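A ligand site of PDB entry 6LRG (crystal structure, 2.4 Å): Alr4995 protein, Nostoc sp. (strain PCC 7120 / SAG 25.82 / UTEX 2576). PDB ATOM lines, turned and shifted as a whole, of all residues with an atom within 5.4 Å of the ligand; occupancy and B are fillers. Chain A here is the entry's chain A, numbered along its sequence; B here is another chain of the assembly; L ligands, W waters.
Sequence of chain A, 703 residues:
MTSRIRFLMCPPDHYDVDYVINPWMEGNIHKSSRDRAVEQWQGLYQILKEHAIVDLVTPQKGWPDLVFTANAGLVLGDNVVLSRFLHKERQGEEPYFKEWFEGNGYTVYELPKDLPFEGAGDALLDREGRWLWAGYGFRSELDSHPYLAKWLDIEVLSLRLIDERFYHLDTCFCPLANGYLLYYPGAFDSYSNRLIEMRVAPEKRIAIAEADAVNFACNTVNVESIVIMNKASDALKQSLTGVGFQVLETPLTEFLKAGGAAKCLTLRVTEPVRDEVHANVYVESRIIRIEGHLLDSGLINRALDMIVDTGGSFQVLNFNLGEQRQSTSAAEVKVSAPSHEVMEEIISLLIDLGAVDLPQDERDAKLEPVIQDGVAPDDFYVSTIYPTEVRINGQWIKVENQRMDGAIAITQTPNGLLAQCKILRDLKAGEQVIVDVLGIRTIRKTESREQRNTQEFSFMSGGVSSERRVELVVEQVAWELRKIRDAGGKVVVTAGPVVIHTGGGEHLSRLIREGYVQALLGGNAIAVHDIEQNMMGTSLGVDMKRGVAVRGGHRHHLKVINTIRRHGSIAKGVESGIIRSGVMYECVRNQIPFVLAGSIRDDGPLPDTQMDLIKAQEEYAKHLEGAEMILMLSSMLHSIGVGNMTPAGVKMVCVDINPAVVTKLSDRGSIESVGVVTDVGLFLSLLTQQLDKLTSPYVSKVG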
ATOM      1  N   GLY A 496      12.507   7.339  11.721  1.00  0.00           N
ATOM      2  CA  GLY A 496      12.396   6.087  10.994  1.00  0.00           C
ATOM      3  C   GLY A 496      11.016   5.976  10.398  1.00  0.00           C
ATOM      4  O   GLY A 496      10.141   6.794  10.677  1.00  0.00           O
ATOM      5  N   PRO A 497      10.803   4.947   9.555  1.00  0.00           N
ATOM      6  CA  PRO A 497       9.535   4.758   8.834  1.00  0.00           C
ATOM      7  C   PRO A 497       8.318   4.494   9.724  1.00  0.00           C
ATOM      8  O   PRO A 497       7.191   4.583   9.266  1.00  0.00           O
ATOM      9  CB  PRO A 497       9.821   3.533   7.943  1.00  0.00           C
ATOM     10  CG  PRO A 497      10.932   2.809   8.647  1.00  0.00           C
ATOM     11  CD  PRO A 497      11.792   3.914   9.222  1.00  0.00           C
ATOM     12  N   VAL A 498       8.532   4.154  10.986  1.00  0.00           N
ATOM     13  CA  VAL A 498       7.400   3.963  11.893  1.00  0.00           C
ATOM     14  C   VAL A 498       6.610   5.255  12.094  1.00  0.00           C
ATOM     15  O   VAL A 498       5.408   5.207  12.303  1.00  0.00           O
ATOM     16  CB  VAL A 498       7.873   3.410  13.227  1.00  0.00           C
ATOM     17  CG1 VAL A 498       6.802   3.572  14.291  1.00  0.00           C
ATOM     18  CG2 VAL A 498       8.235   1.947  13.068  1.00  0.00           C
ATOM     19  N   THR A 502       2.642   4.408  11.700  1.00  0.00           N
ATOM     20  CA  THR A 502       1.716   4.564  12.797  1.00  0.00           C
ATOM     21  C   THR A 502       0.667   5.667  12.510  1.00  0.00           C
ATOM     22  O   THR A 502      -0.405   5.705  13.160  1.00  0.00           O
ATOM     23  CB  THR A 502       2.495   4.856  14.090  1.00  0.00           C
ATOM     24  OG1 THR A 502       1.655   4.566  15.211  1.00  0.00           O
ATOM     25  CG2 THR A 502       2.968   6.307  14.130  1.00  0.00           C
ATOM     26  N   GLY A 523      16.514   7.407   6.424  1.00  0.00           N
ATOM     27  CA  GLY A 523      16.891   6.309   5.569  1.00  0.00           C
ATOM     28  C   GLY A 523      15.990   6.254   4.353  1.00  0.00           C
ATOM     29  O   GLY A 523      15.102   7.094   4.166  1.00  0.00           O
ATOM     30  N   ASN A 524      16.222   5.244   3.535  1.00  0.00           N
ATOM     31  CA  ASN A 524      15.470   5.028   2.319  1.00  0.00           C
ATOM     32  C   ASN A 524      13.993   4.821   2.613  1.00  0.00           C
ATOM     33  O   ASN A 524      13.124   5.371   1.936  1.00  0.00           O
ATOM     34  CB  ASN A 524      16.039   3.824   1.572  1.00  0.00           C
ATOM     35  CG  ASN A 524      15.552   3.740   0.154  1.00  0.00           C
ATOM     36  OD1 ASN A 524      16.061   4.449  -0.724  1.00  0.00           O
ATOM     37  ND2 ASN A 524      14.558   2.901  -0.088  1.00  0.00           N
ATOM     38  N   ALA A 525      13.719   4.027   3.637  1.00  0.00           N
ATOM     39  CA  ALA A 525      12.359   3.630   3.989  1.00  0.00           C
ATOM     40  C   ALA A 525      11.425   4.774   4.326  1.00  0.00           C
ATOM     41  O   ALA A 525      10.285   4.755   3.884  1.00  0.00           O
ATOM     42  CB  ALA A 525      12.383   2.692   5.156  1.00  0.00           C
ATOM     43  N   ILE A 526      11.868   5.729   5.147  1.00  0.00           N
ATOM     44  CA  ILE A 526      10.960   6.748   5.603  1.00  0.00           C
ATOM     45  C   ILE A 526      10.532   7.612   4.428  1.00  0.00           C
ATOM     46  O   ILE A 526       9.387   8.056   4.375  1.00  0.00           O
ATOM     47  CB  ILE A 526      11.534   7.660   6.733  1.00  0.00           C
ATOM     48  CG1 ILE A 526      10.495   8.763   7.031  1.00  0.00           C
ATOM     49  CG2 ILE A 526      12.893   8.246   6.336  1.00  0.00           C
ATOM     50  CD1 ILE A 526      10.616   9.472   8.355  1.00  0.00           C
ATOM     51  N   VAL A 528      10.381   6.640   1.174  1.00  0.00           N
ATOM     52  CA  VAL A 528       9.522   5.850   0.303  1.00  0.00           C
ATOM     53  C   VAL A 528       8.082   5.785   0.812  1.00  0.00           C
ATOM     54  O   VAL A 528       7.123   5.992   0.050  1.00  0.00           O
ATOM     55  CB  VAL A 528      10.054   4.402   0.150  1.00  0.00           C
ATOM     56  CG1 VAL A 528       9.070   3.580  -0.645  1.00  0.00           C
ATOM     57  CG2 VAL A 528      11.411   4.413  -0.526  1.00  0.00           C
ATOM     58  N   HIS A 529       7.916   5.529   2.098  1.00  0.00           N
ATOM     59  CA  HIS A 529       6.578   5.393   2.669  1.00  0.00           C
ATOM     60  C   HIS A 529       5.838   6.715   2.826  1.00  0.00           C
ATOM     61  O   HIS A 529       4.628   6.773   2.631  1.00  0.00           O
ATOM     62  CB  HIS A 529       6.667   4.649   3.997  1.00  0.00           C
ATOM     63  CG  HIS A 529       7.079   3.212   3.831  1.00  0.00           C
ATOM     64  ND1 HIS A 529       7.874   2.559   4.734  1.00  0.00           N
ATOM     65  CD2 HIS A 529       6.818   2.327   2.845  1.00  0.00           C
ATOM     66  CE1 HIS A 529       8.080   1.321   4.317  1.00  0.00           C
ATOM     67  NE2 HIS A 529       7.453   1.164   3.172  1.00  0.00           N
ATOM     68  N   HIS A 557       4.170   0.561  -3.074  1.00  0.00           N
ATOM     69  CA  HIS A 557       5.528   0.743  -2.593  1.00  0.00           C
ATOM     70  C   HIS A 557       6.535   0.780  -3.762  1.00  0.00           C
ATOM     71  O   HIS A 557       7.295   1.738  -3.926  1.00  0.00           O
ATOM     72  CB  HIS A 557       5.766  -0.426  -1.624  1.00  0.00           C
ATOM     73  CG  HIS A 557       7.126  -0.474  -1.016  1.00  0.00           C
ATOM     74  ND1 HIS A 557       7.669   0.601  -0.346  1.00  0.00           N
ATOM     75  CD2 HIS A 557       8.023  -1.478  -0.926  1.00  0.00           C
ATOM     76  CE1 HIS A 557       8.871   0.264   0.110  1.00  0.00           C
ATOM     77  NE2 HIS A 557       9.105  -0.993  -0.239  1.00  0.00           N
ATOM     78  N   ILE A 561       9.012   3.844  -5.804  1.00  0.00           N
ATOM     79  CA  ILE A 561      10.447   3.742  -6.011  1.00  0.00           C
ATOM     80  C   ILE A 561      10.799   3.870  -7.480  1.00  0.00           C
ATOM     81  O   ILE A 561      11.778   4.529  -7.843  1.00  0.00           O
ATOM     82  CB  ILE A 561      11.004   2.401  -5.479  1.00  0.00           C
ATOM     83  CG1 ILE A 561      10.965   2.364  -3.953  1.00  0.00           C
ATOM     84  CG2 ILE A 561      12.430   2.202  -5.933  1.00  0.00           C
ATOM     85  CD1 ILE A 561      11.063   0.975  -3.374  1.00  0.00           C
ATOM     86  N   ALA A 597      20.474   7.862   4.566  1.00  0.00           N
ATOM     87  CA  ALA A 597      21.560   6.886   4.680  1.00  0.00           C
ATOM     88  C   ALA A 597      21.058   5.506   4.302  1.00  0.00           C
ATOM     89  O   ALA A 597      19.994   5.096   4.762  1.00  0.00           O
ATOM     90  CB  ALA A 597      22.142   6.884   6.099  1.00  0.00           C
ATOM     91  N   GLY A 598      21.811   4.815   3.459  1.00  0.00           N
ATOM     92  CA  GLY A 598      21.401   3.484   3.010  1.00  0.00           C
ATOM     93  C   GLY A 598      21.521   2.393   4.061  1.00  0.00           C
ATOM     94  O   GLY A 598      22.205   2.544   5.069  1.00  0.00           O
ATOM     95  N   SER A 599      20.870   1.264   3.795  1.00  0.00           N
ATOM     96  CA  SER A 599      20.978   0.082   4.649  1.00  0.00           C
ATOM     97  C   SER A 599      20.901  -1.166   3.782  1.00  0.00           C
ATOM     98  O   SER A 599      20.523  -1.087   2.601  1.00  0.00           O
ATOM     99  CB  SER A 599      19.883   0.043   5.698  1.00  0.00           C
ATOM    100  OG  SER A 599      18.750  -0.678   5.198  1.00  0.00           O
ATOM    101  N   ARG A 601      18.850  -3.593   3.815  1.00  0.00           N
ATOM    102  CA  ARG A 601      17.536  -4.040   3.395  1.00  0.00           C
ATOM    103  C   ARG A 601      16.821  -3.061   2.451  1.00  0.00           C
ATOM    104  O   ARG A 601      15.648  -3.263   2.120  1.00  0.00           O
ATOM    105  CB  ARG A 601      16.668  -4.328   4.610  1.00  0.00           C
ATOM    106  CG  ARG A 601      16.378  -3.135   5.465  1.00  0.00           C
ATOM    107  CD  ARG A 601      15.130  -3.405   6.291  1.00  0.00           C
ATOM    108  NE  ARG A 601      13.971  -3.652   5.434  1.00  0.00           N
ATOM    109  CZ  ARG A 601      12.713  -3.745   5.871  1.00  0.00           C
ATOM    110  NH1 ARG A 601      12.458  -3.587   7.162  1.00  0.00           N
ATOM    111  NH2 ARG A 601      11.723  -3.981   5.006  1.00  0.00           N
ATOM    112  N   ASP A 602      17.513  -2.024   1.984  1.00  0.00           N
ATOM    113  CA  ASP A 602      16.880  -1.045   1.103  1.00  0.00           C
ATOM    114  C   ASP A 602      16.347  -1.609  -0.208  1.00  0.00           C
ATOM    115  O   ASP A 602      17.040  -2.324  -0.936  1.00  0.00           O
ATOM    116  CB  ASP A 602      17.846   0.084   0.751  1.00  0.00           C
ATOM    117  CG  ASP A 602      18.196   0.965   1.945  1.00  0.00           C
ATOM    118  OD1 ASP A 602      17.615   0.805   3.052  1.00  0.00           O
ATOM    119  OD2 ASP A 602      19.062   1.837   1.751  1.00  0.00           O
ATOM    120  N   ASP A 603      15.102  -1.256  -0.514  1.00  0.00           N
ATOM    121  CA  ASP A 603      14.520  -1.555  -1.813  1.00  0.00           C
ATOM    122  C   ASP A 603      14.831  -0.415  -2.766  1.00  0.00           C
ATOM    123  O   ASP A 603      14.632   0.745  -2.413  1.00  0.00           O
ATOM    124  CB  ASP A 603      13.006  -1.768  -1.689  1.00  0.00           C
ATOM    125  CG  ASP A 603      12.673  -3.035  -0.912  1.00  0.00           C
ATOM    126  OD1 ASP A 603      13.366  -4.065  -1.099  1.00  0.00           O
ATOM    127  OD2 ASP A 603      11.726  -2.988  -0.088  1.00  0.00           O
ATOM    128  N   SER A 634      11.598   7.254  16.977  1.00  0.00           N
ATOM    129  CA  SER A 634      11.452   5.832  16.683  1.00  0.00           C
ATOM    130  C   SER A 634      12.439   5.314  15.637  1.00  0.00           C
ATOM    131  O   SER A 634      12.020   4.804  14.593  1.00  0.00           O
ATOM    132  CB  SER A 634      10.034   5.539  16.220  1.00  0.00           C
ATOM    133  OG  SER A 634       9.794   6.179  14.969  1.00  0.00           O
ATOM    134  N   SER A 635      13.729   5.431  15.909  1.00  0.00           N
ATOM    135  CA  SER A 635      14.729   4.961  14.962  1.00  0.00           C
ATOM    136  C   SER A 635      15.999   4.546  15.669  1.00  0.00           C
ATOM    137  O   SER A 635      16.934   5.342  15.792  1.00  0.00           O
ATOM    138  CB  SER A 635      15.044   6.043  13.934  1.00  0.00           C
ATOM    139  OG  SER A 635      16.000   5.555  13.013  1.00  0.00           O
ATOM    140  N   MET A 636      16.044   3.304  16.140  1.00  0.00           N
ATOM    141  CA  MET A 636      17.182   2.811  16.883  1.00  0.00           C
ATOM    142  C   MET A 636      18.501   2.943  16.104  1.00  0.00           C
ATOM    143  O   MET A 636      19.453   3.519  16.611  1.00  0.00           O
ATOM    144  CB  MET A 636      16.961   1.342  17.301  1.00  0.00           C
ATOM    145  CG  MET A 636      17.840   0.887  18.456  1.00  0.00           C
ATOM    146  SD  MET A 636      17.670  -0.870  18.795  1.00  0.00           S
ATOM    147  CE  MET A 636      18.685  -1.040  20.263  1.00  0.00           C
ATOM    148  N   LEU A 637      18.555   2.420  14.881  1.00  0.00           N
ATOM    149  CA  LEU A 637      19.818   2.382  14.161  1.00  0.00           C
ATOM    150  C   LEU A 637      20.358   3.780  13.905  1.00  0.00           C
ATOM    151  O   LEU A 637      21.558   4.026  14.024  1.00  0.00           O
ATOM    152  CB  LEU A 637      19.664   1.632  12.839  1.00  0.00           C
ATOM    153  CG  LEU A 637      20.896   1.541  11.929  1.00  0.00           C
ATOM    154  CD1 LEU A 637      21.763   0.323  12.266  1.00  0.00           C
ATOM    155  CD2 LEU A 637      20.483   1.546  10.460  1.00  0.00           C
ATOM    156  N   HIS A 638      19.451   4.711  13.585  1.00  0.00           N
ATOM    157  CA  HIS A 638      19.851   6.071  13.226  1.00  0.00           C
ATOM    158  C   HIS A 638      20.061   6.947  14.440  1.00  0.00           C
ATOM    159  O   HIS A 638      20.959   7.784  14.455  1.00  0.00           O
ATOM    160  CB  HIS A 638      18.821   6.701  12.279  1.00  0.00           C
ATOM    161  CG  HIS A 638      18.794   6.050  10.925  1.00  0.00           C
ATOM    162  ND1 HIS A 638      19.307   6.657   9.808  1.00  0.00           N
ATOM    163  CD2 HIS A 638      18.353   4.840  10.532  1.00  0.00           C
ATOM    164  CE1 HIS A 638      19.176   5.847   8.773  1.00  0.00           C
ATOM    165  NE2 HIS A 638      18.597   4.733   9.181  1.00  0.00           N
ATOM    166  N   VAL A 655      12.207   9.233  21.411  1.00  0.00           N
ATOM    167  CA  VAL A 655      10.847   8.710  21.463  1.00  0.00           C
ATOM    168  C   VAL A 655      10.759   7.308  20.859  1.00  0.00           C
ATOM    169  O   VAL A 655      11.062   7.105  19.684  1.00  0.00           O
ATOM    170  CB  VAL A 655       9.854   9.635  20.742  1.00  0.00           C
ATOM    171  CG1 VAL A 655       8.433   9.219  21.055  1.00  0.00           C
ATOM    172  CG2 VAL A 655      10.085  11.080  21.159  1.00  0.00           C
ATOM    173  N   ASP A 656      10.341   6.348  21.670  1.00  0.00           N
ATOM    174  CA  ASP A 656      10.290   4.953  21.236  1.00  0.00           C
ATOM    175  C   ASP A 656       9.347   4.171  22.137  1.00  0.00           C
ATOM    176  O   ASP A 656       9.183   4.508  23.308  1.00  0.00           O
ATOM    177  CB  ASP A 656      11.694   4.347  21.271  1.00  0.00           C
ATOM    178  CG  ASP A 656      11.822   3.117  20.386  1.00  0.00           C
ATOM    179  OD1 ASP A 656      11.366   2.013  20.788  1.00  0.00           O
ATOM    180  OD2 ASP A 656      12.417   3.254  19.298  1.00  0.00           O
ATOM    181  N   ILE A 657       8.738   3.119  21.601  1.00  0.00           N
ATOM    182  CA  ILE A 657       7.823   2.284  22.381  1.00  0.00           C
ATOM    183  C   ILE A 657       8.549   1.207  23.207  1.00  0.00           C
ATOM    184  O   ILE A 657       7.987   0.684  24.179  1.00  0.00           O
ATOM    185  CB  ILE A 657       6.785   1.607  21.464  1.00  0.00           C
ATOM    186  CG1 ILE A 657       5.571   1.179  22.279  1.00  0.00           C
ATOM    187  CG2 ILE A 657       7.407   0.458  20.669  1.00  0.00           C
ATOM    188  CD1 ILE A 657       4.830   2.362  22.927  1.00  0.00           C
ATOM    189  N   ASN A 658       9.786   0.884  22.835  1.00  0.00           N
ATOM    190  CA  ASN A 658      10.610  -0.088  23.557  1.00  0.00           C
ATOM    191  C   ASN A 658      11.401   0.604  24.659  1.00  0.00           C
ATOM    192  O   ASN A 658      12.236   1.464  24.375  1.00  0.00           O
ATOM    193  CB  ASN A 658      11.560  -0.818  22.599  1.00  0.00           C
ATOM    194  CG  ASN A 658      12.466  -1.841  23.307  1.00  0.00           C
ATOM    195  OD1 ASN A 658      12.933  -1.616  24.423  1.00  0.00           O
ATOM    196  ND2 ASN A 658      12.727  -2.946  22.630  1.00  0.00           N
ATOM    197  N   VAL A 661      15.451   0.599  24.287  1.00  0.00           N
ATOM    198  CA  VAL A 661      16.040   1.577  23.380  1.00  0.00           C
ATOM    199  C   VAL A 661      16.197   2.976  24.011  1.00  0.00           C
ATOM    200  O   VAL A 661      17.245   3.617  23.902  1.00  0.00           O
ATOM    201  CB  VAL A 661      15.205   1.734  22.111  1.00  0.00           C
ATOM    202  CG1 VAL A 661      15.960   2.564  21.092  1.00  0.00           C
ATOM    203  CG2 VAL A 661      14.854   0.368  21.545  1.00  0.00           C
ATOM    204  N   THR A 678       6.424   5.756  24.400  1.00  0.00           N
ATOM    205  CA  THR A 678       5.059   6.001  23.925  1.00  0.00           C
ATOM    206  C   THR A 678       5.071   5.814  22.403  1.00  0.00           C
ATOM    207  O   THR A 678       6.141   5.715  21.803  1.00  0.00           O
ATOM    208  CB  THR A 678       4.561   7.429  24.305  1.00  0.00           C
ATOM    209  OG1 THR A 678       3.141   7.529  24.151  1.00  0.00           O
ATOM    210  CG2 THR A 678       5.223   8.483  23.459  1.00  0.00           C
ATOM    211  N   ASP A 679       3.900   5.747  21.798  1.00  0.00           N
ATOM    212  CA  ASP A 679       3.812   5.693  20.346  1.00  0.00           C
ATOM    213  C   ASP A 679       4.261   7.034  19.752  1.00  0.00           C
ATOM    214  O   ASP A 679       3.752   8.087  20.137  1.00  0.00           O
ATOM    215  CB  ASP A 679       2.377   5.359  19.899  1.00  0.00           C
ATOM    216  CG  ASP A 679       2.185   5.550  18.400  1.00  0.00           C
ATOM    217  OD1 ASP A 679       2.519   4.620  17.641  1.00  0.00           O
ATOM    218  OD2 ASP A 679       1.707   6.630  17.970  1.00  0.00           O
ATOM    219  N   VAL A 680       5.190   6.991  18.812  1.00  0.00           N
ATOM    220  CA  VAL A 680       5.749   8.231  18.278  1.00  0.00           C
ATOM    221  C   VAL A 680       4.703   9.099  17.593  1.00  0.00           C
ATOM    222  O   VAL A 680       4.799  10.326  17.611  1.00  0.00           O
ATOM    223  CB  VAL A 680       6.900   7.955  17.300  1.00  0.00           C
ATOM    224  CG1 VAL A 680       6.380   7.258  16.045  1.00  0.00           C
ATOM    225  CG2 VAL A 680       7.618   9.249  16.952  1.00  0.00           C
ATOM    226  N   GLY A 681       3.663   8.476  17.033  1.00  0.00           N
ATOM    227  CA  GLY A 681       2.604   9.237  16.377  1.00  0.00           C
ATOM    228  C   GLY A 681       1.800  10.066  17.367  1.00  0.00           C
ATOM    229  O   GLY A 681       1.600  11.262  17.164  1.00  0.00           O
ATOM    230  N   MET B 636      17.438  -8.684  13.268  1.00  0.00           N
ATOM    231  CA  MET B 636      16.365  -7.855  12.707  1.00  0.00           C
ATOM    232  C   MET B 636      16.659  -7.206  11.343  1.00  0.00           C
ATOM    233  O   MET B 636      16.075  -7.590  10.343  1.00  0.00           O
ATOM    234  CB  MET B 636      15.981  -6.770  13.695  1.00  0.00           C
ATOM    235  CG  MET B 636      14.525  -6.350  13.563  1.00  0.00           C
ATOM    236  SD  MET B 636      14.276  -4.556  13.426  1.00  0.00           S
ATOM    237  CE  MET B 636      14.860  -4.232  11.758  1.00  0.00           C
ATOM    238  N   LEU B 637      17.555  -6.241  11.309  1.00  0.00           N
ATOM    239  CA  LEU B 637      17.835  -5.532  10.063  1.00  0.00           C
ATOM    240  C   LEU B 637      18.399  -6.463   8.994  1.00  0.00           C
ATOM    241  O   LEU B 637      17.980  -6.438   7.832  1.00  0.00           O
ATOM    242  CB  LEU B 637      18.803  -4.377  10.335  1.00  0.00           C
ATOM    243  CG  LEU B 637      19.451  -3.658   9.168  1.00  0.00           C
ATOM    244  CD1 LEU B 637      18.431  -2.767   8.470  1.00  0.00           C
ATOM    245  CD2 LEU B 637      20.670  -2.845   9.654  1.00  0.00           C
HETATM  246  P1  LIG L   1      15.024   0.171  14.002  1.00  0.00           P
HETATM  247  O1  LIG L   1      16.095   1.166  14.289  1.00  0.00           O
HETATM  248  O2  LIG L   1      15.571  -1.228  14.309  1.00  0.00           O
HETATM  249  O3  LIG L   1      13.713   0.336  14.922  1.00  0.00           O
HETATM  250  C1  LIG L   1      13.133   1.622  15.153  1.00  0.00           C
HETATM  251  C2  LIG L   1      12.573   1.699  16.601  1.00  0.00           C
HETATM  252  O4  LIG L   1      11.054   2.084  16.529  1.00  0.00           O
HETATM  253  C3  LIG L   1      12.623   0.587  17.197  1.00  0.00           C
HETATM  254  O5  LIG L   1      13.515   0.675  18.362  1.00  0.00           O
HETATM  255  C4  LIG L   1      11.086   0.247  17.758  1.00  0.00           C
HETATM  256  O6  LIG L   1      11.200  -0.244  19.127  1.00  0.00           O
HETATM  257  C5  LIG L   1      10.445   1.347  17.734  1.00  0.00           C
HETATM  258  N1  LIG L   1       8.975   1.184  17.441  1.00  0.00           N
HETATM  259  C6  LIG L   1       8.145   0.280  16.860  1.00  0.00           C
HETATM  260  N2  LIG L   1       6.877   0.800  16.896  1.00  0.00           N
HETATM  261  C7  LIG L   1       6.930   2.017  17.482  1.00  0.00           C
HETATM  262  C8  LIG L   1       5.943   2.971  17.759  1.00  0.00           C
HETATM  263  N3  LIG L   1       4.531   3.042  17.553  1.00  0.00           N
HETATM  264  N4  LIG L   1       6.259   4.140  18.367  1.00  0.00           N
HETATM  265  C9  LIG L   1       7.562   4.405  18.710  1.00  0.00           C
HETATM  266  N5  LIG L   1       8.563   3.471  18.435  1.00  0.00           N
HETATM  267  C10 LIG L   1       8.238   2.273  17.826  1.00  0.00           C
HETATM  268  O7  LIG L   1      14.623   0.290  12.417  1.00  0.00           O
HETATM  269  P2  LIG L   1      14.633   1.631  11.512  1.00  0.00           P
HETATM  270  O8  LIG L   1      13.209   2.076  11.359  1.00  0.00           O
HETATM  271  O9  LIG L   1      15.447   2.786  12.114  1.00  0.00           O
HETATM  272  O10 LIG L   1      15.203   1.249  10.076  1.00  0.00           O
HETATM  273  C11 LIG L   1      16.289   0.329   9.933  1.00  0.00           C
HETATM  274  C12 LIG L   1      16.929   0.575   8.547  1.00  0.00           C
HETATM  275  O11 LIG L   1      16.393  -0.238   7.649  1.00  0.00           O
HETATM  276  C13 LIG L   1      16.599   2.003   8.119  1.00  0.00           C
HETATM  277  O12 LIG L   1      17.711   2.754   7.790  1.00  0.00           O
HETATM  278  C14 LIG L   1      15.630   1.816   6.897  1.00  0.00           C
HETATM  279  O13 LIG L   1      15.677   2.945   5.919  1.00  0.00           O
HETATM  280  C15 LIG L   1      15.959   0.683   6.368  1.00  0.00           C
HETATM  281  N6  LIG L   1      14.792   0.223   5.635  1.00  0.00           N
HETATM  282  C16 LIG L   1      14.642   0.422   4.234  1.00  0.00           C
HETATM  283  C17 LIG L   1      13.449  -0.012   3.590  1.00  0.00           C
HETATM  284  C18 LIG L   1      13.145   0.171   2.067  1.00  0.00           C
HETATM  285  O14 LIG L   1      13.998   0.502   1.248  1.00  0.00           O
HETATM  286  N7  LIG L   1      11.788  -0.005   1.614  1.00  0.00           N
HETATM  287  C19 LIG L   1      12.447  -0.611   4.346  1.00  0.00           C
HETATM  288  C20 LIG L   1      12.601  -0.778   5.719  1.00  0.00           C
HETATM  289  C21 LIG L   1      13.785  -0.359   6.366  1.00  0.00           C
HETATM  290  O   HOH W   1      11.194   3.286  12.333  1.00  0.00           O
HETATM  291  O   HOH W   2       9.502  -0.324   6.913  1.00  0.00           O
HETATM  292  O   HOH W   3      18.139   3.338   4.514  1.00  0.00           O
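OD2 of Asp 602 sits at hydrogen-bond distance from N of Ser 599, 2.8 Å away.
N of Val 661 lies within hydrogen-bond range of OD1 of Asn 658, at 3.4 Å.
The side-chain amide nitrogen (ND2) of Asn 524 lies within hydrogen-bond range of the backbone carbonyl oxygen (O) of Asp 603, at 3.2 Å.
N of Arg 601 lies close to OG of Ser 599 (3.2 Å).
ND1 of His 529 is in hydrogen-bond range of O of Ala 525 (3.4 Å).
The side-chain carboxylate of Asp 603 is in hydrogen-bond range of a ring nitrogen (NE2) of His 557 (3.3 Å).
The side-chain carboxylate (OD1) of Asp 679 is in hydrogen-bond range of the side-chain hydroxyl (OG1) of Thr 502, at 2.6 Å.
The backbone carbonyl oxygen (O) of Val 655 sits at hydrogen-bond distance from the backbone NH (N) of Ser 634 (2.8 Å).
N3 of the ligand lies within hydrogen-bond range of OD1 of Asp 679, at 2.6 Å.
The backbone NH of Ala 525 is in hydrogen-bond range of an oxygen (O13) of the ligand (3.2 Å).
N of Asp 603 is in hydrogen-bond range of O14 of the ligand (2.7 Å).
The backbone NH (N) of Val 680 sits at hydrogen-bond distance from a nitrogen (N4) of the ligand, at 3.1 Å.
O1 of the ligand lies within hydrogen-bond range of N of Met 636 of chain A.
The side-chain hydroxyl of Ser 599 lies close to an oxygen (O11) of the ligand, 3.4 Å away.
The side-chain carboxylate of Asp 603 sits at hydrogen-bond distance from a nitrogen (N7) of the ligand.
The backbone NH of Ile 657 sits at hydrogen-bond distance from a nitrogen (N5) of the ligand (3.2 Å).
The side-chain hydroxyl (OG) of Ser 635 lies within hydrogen-bond range of an oxygen (O9) of the ligand.
The backbone NH (N) of Asn 524 lies within hydrogen-bond range of an oxygen (O13) of the ligand, at 3.4 Å.
The backbone NH (N) of Leu 637 of chain A sits at hydrogen-bond distance from an oxygen (O1) of the ligand (2.8 Å).
A ring nitrogen (NE2) of His 557 sits close to a nitrogen (N7) of the ligand (3.4 Å).
OD1 of Asp 656 sits at hydrogen-bond distance from O6 of the ligand (2.8 Å).
An oxygen (O12) of the ligand sits at hydrogen-bond distance from a ring nitrogen (NE2) of His 638 (2.6 Å).
An oxygen (O14) of the ligand is in hydrogen-bond range of the side-chain amide nitrogen (ND2) of Asn 524 (2.8 Å).
Water W1 lies within hydrogen-bond range of O8 of the ligand (2.5 Å), O of Ser 634 (2.8 Å) and N of Val 498 (3.1 Å).
Water W3 lies within hydrogen-bond range of the backbone carbonyl oxygen of Ala 597 (2.6 Å), an oxygen (O13) of the ligand (2.9 Å), the backbone NH of Asn 524 (2.9 Å) and the side-chain carboxylate of Asp 602 (3.0 Å).
An oxygen (O4) of the ligand lies close to the backbone carbonyl oxygen (O) of Ser 634, 3.5 Å away.
O2 of the ligand lies close to SD of Met 636 of chain B (3.7 Å).
Merely in contact with the ligand: Arg 601, Pro 497, Asp 602, Leu 637 of chain B, Val 661, Asn 658, Val 498, Gly 523 and Thr 678.
24 residues have an atom within 4 Å of the ligand: Pro 497, Val 498, Gly 523, Asn 524, Ala 525, His 557, Ser 599, Arg 601, Asp 602, Asp 603, Ser 634, Ser 635, Met 636 of chain A, Leu 637 of chain A, His 638, Asp 656, Ile 657, Asn 658, Val 661, Thr 678, Asp 679, Val 680, Met 636 of chain B and Leu 637 of chain B.
The nearest printed residue that does not touch the ligand is Thr 502 (4.01 Å).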
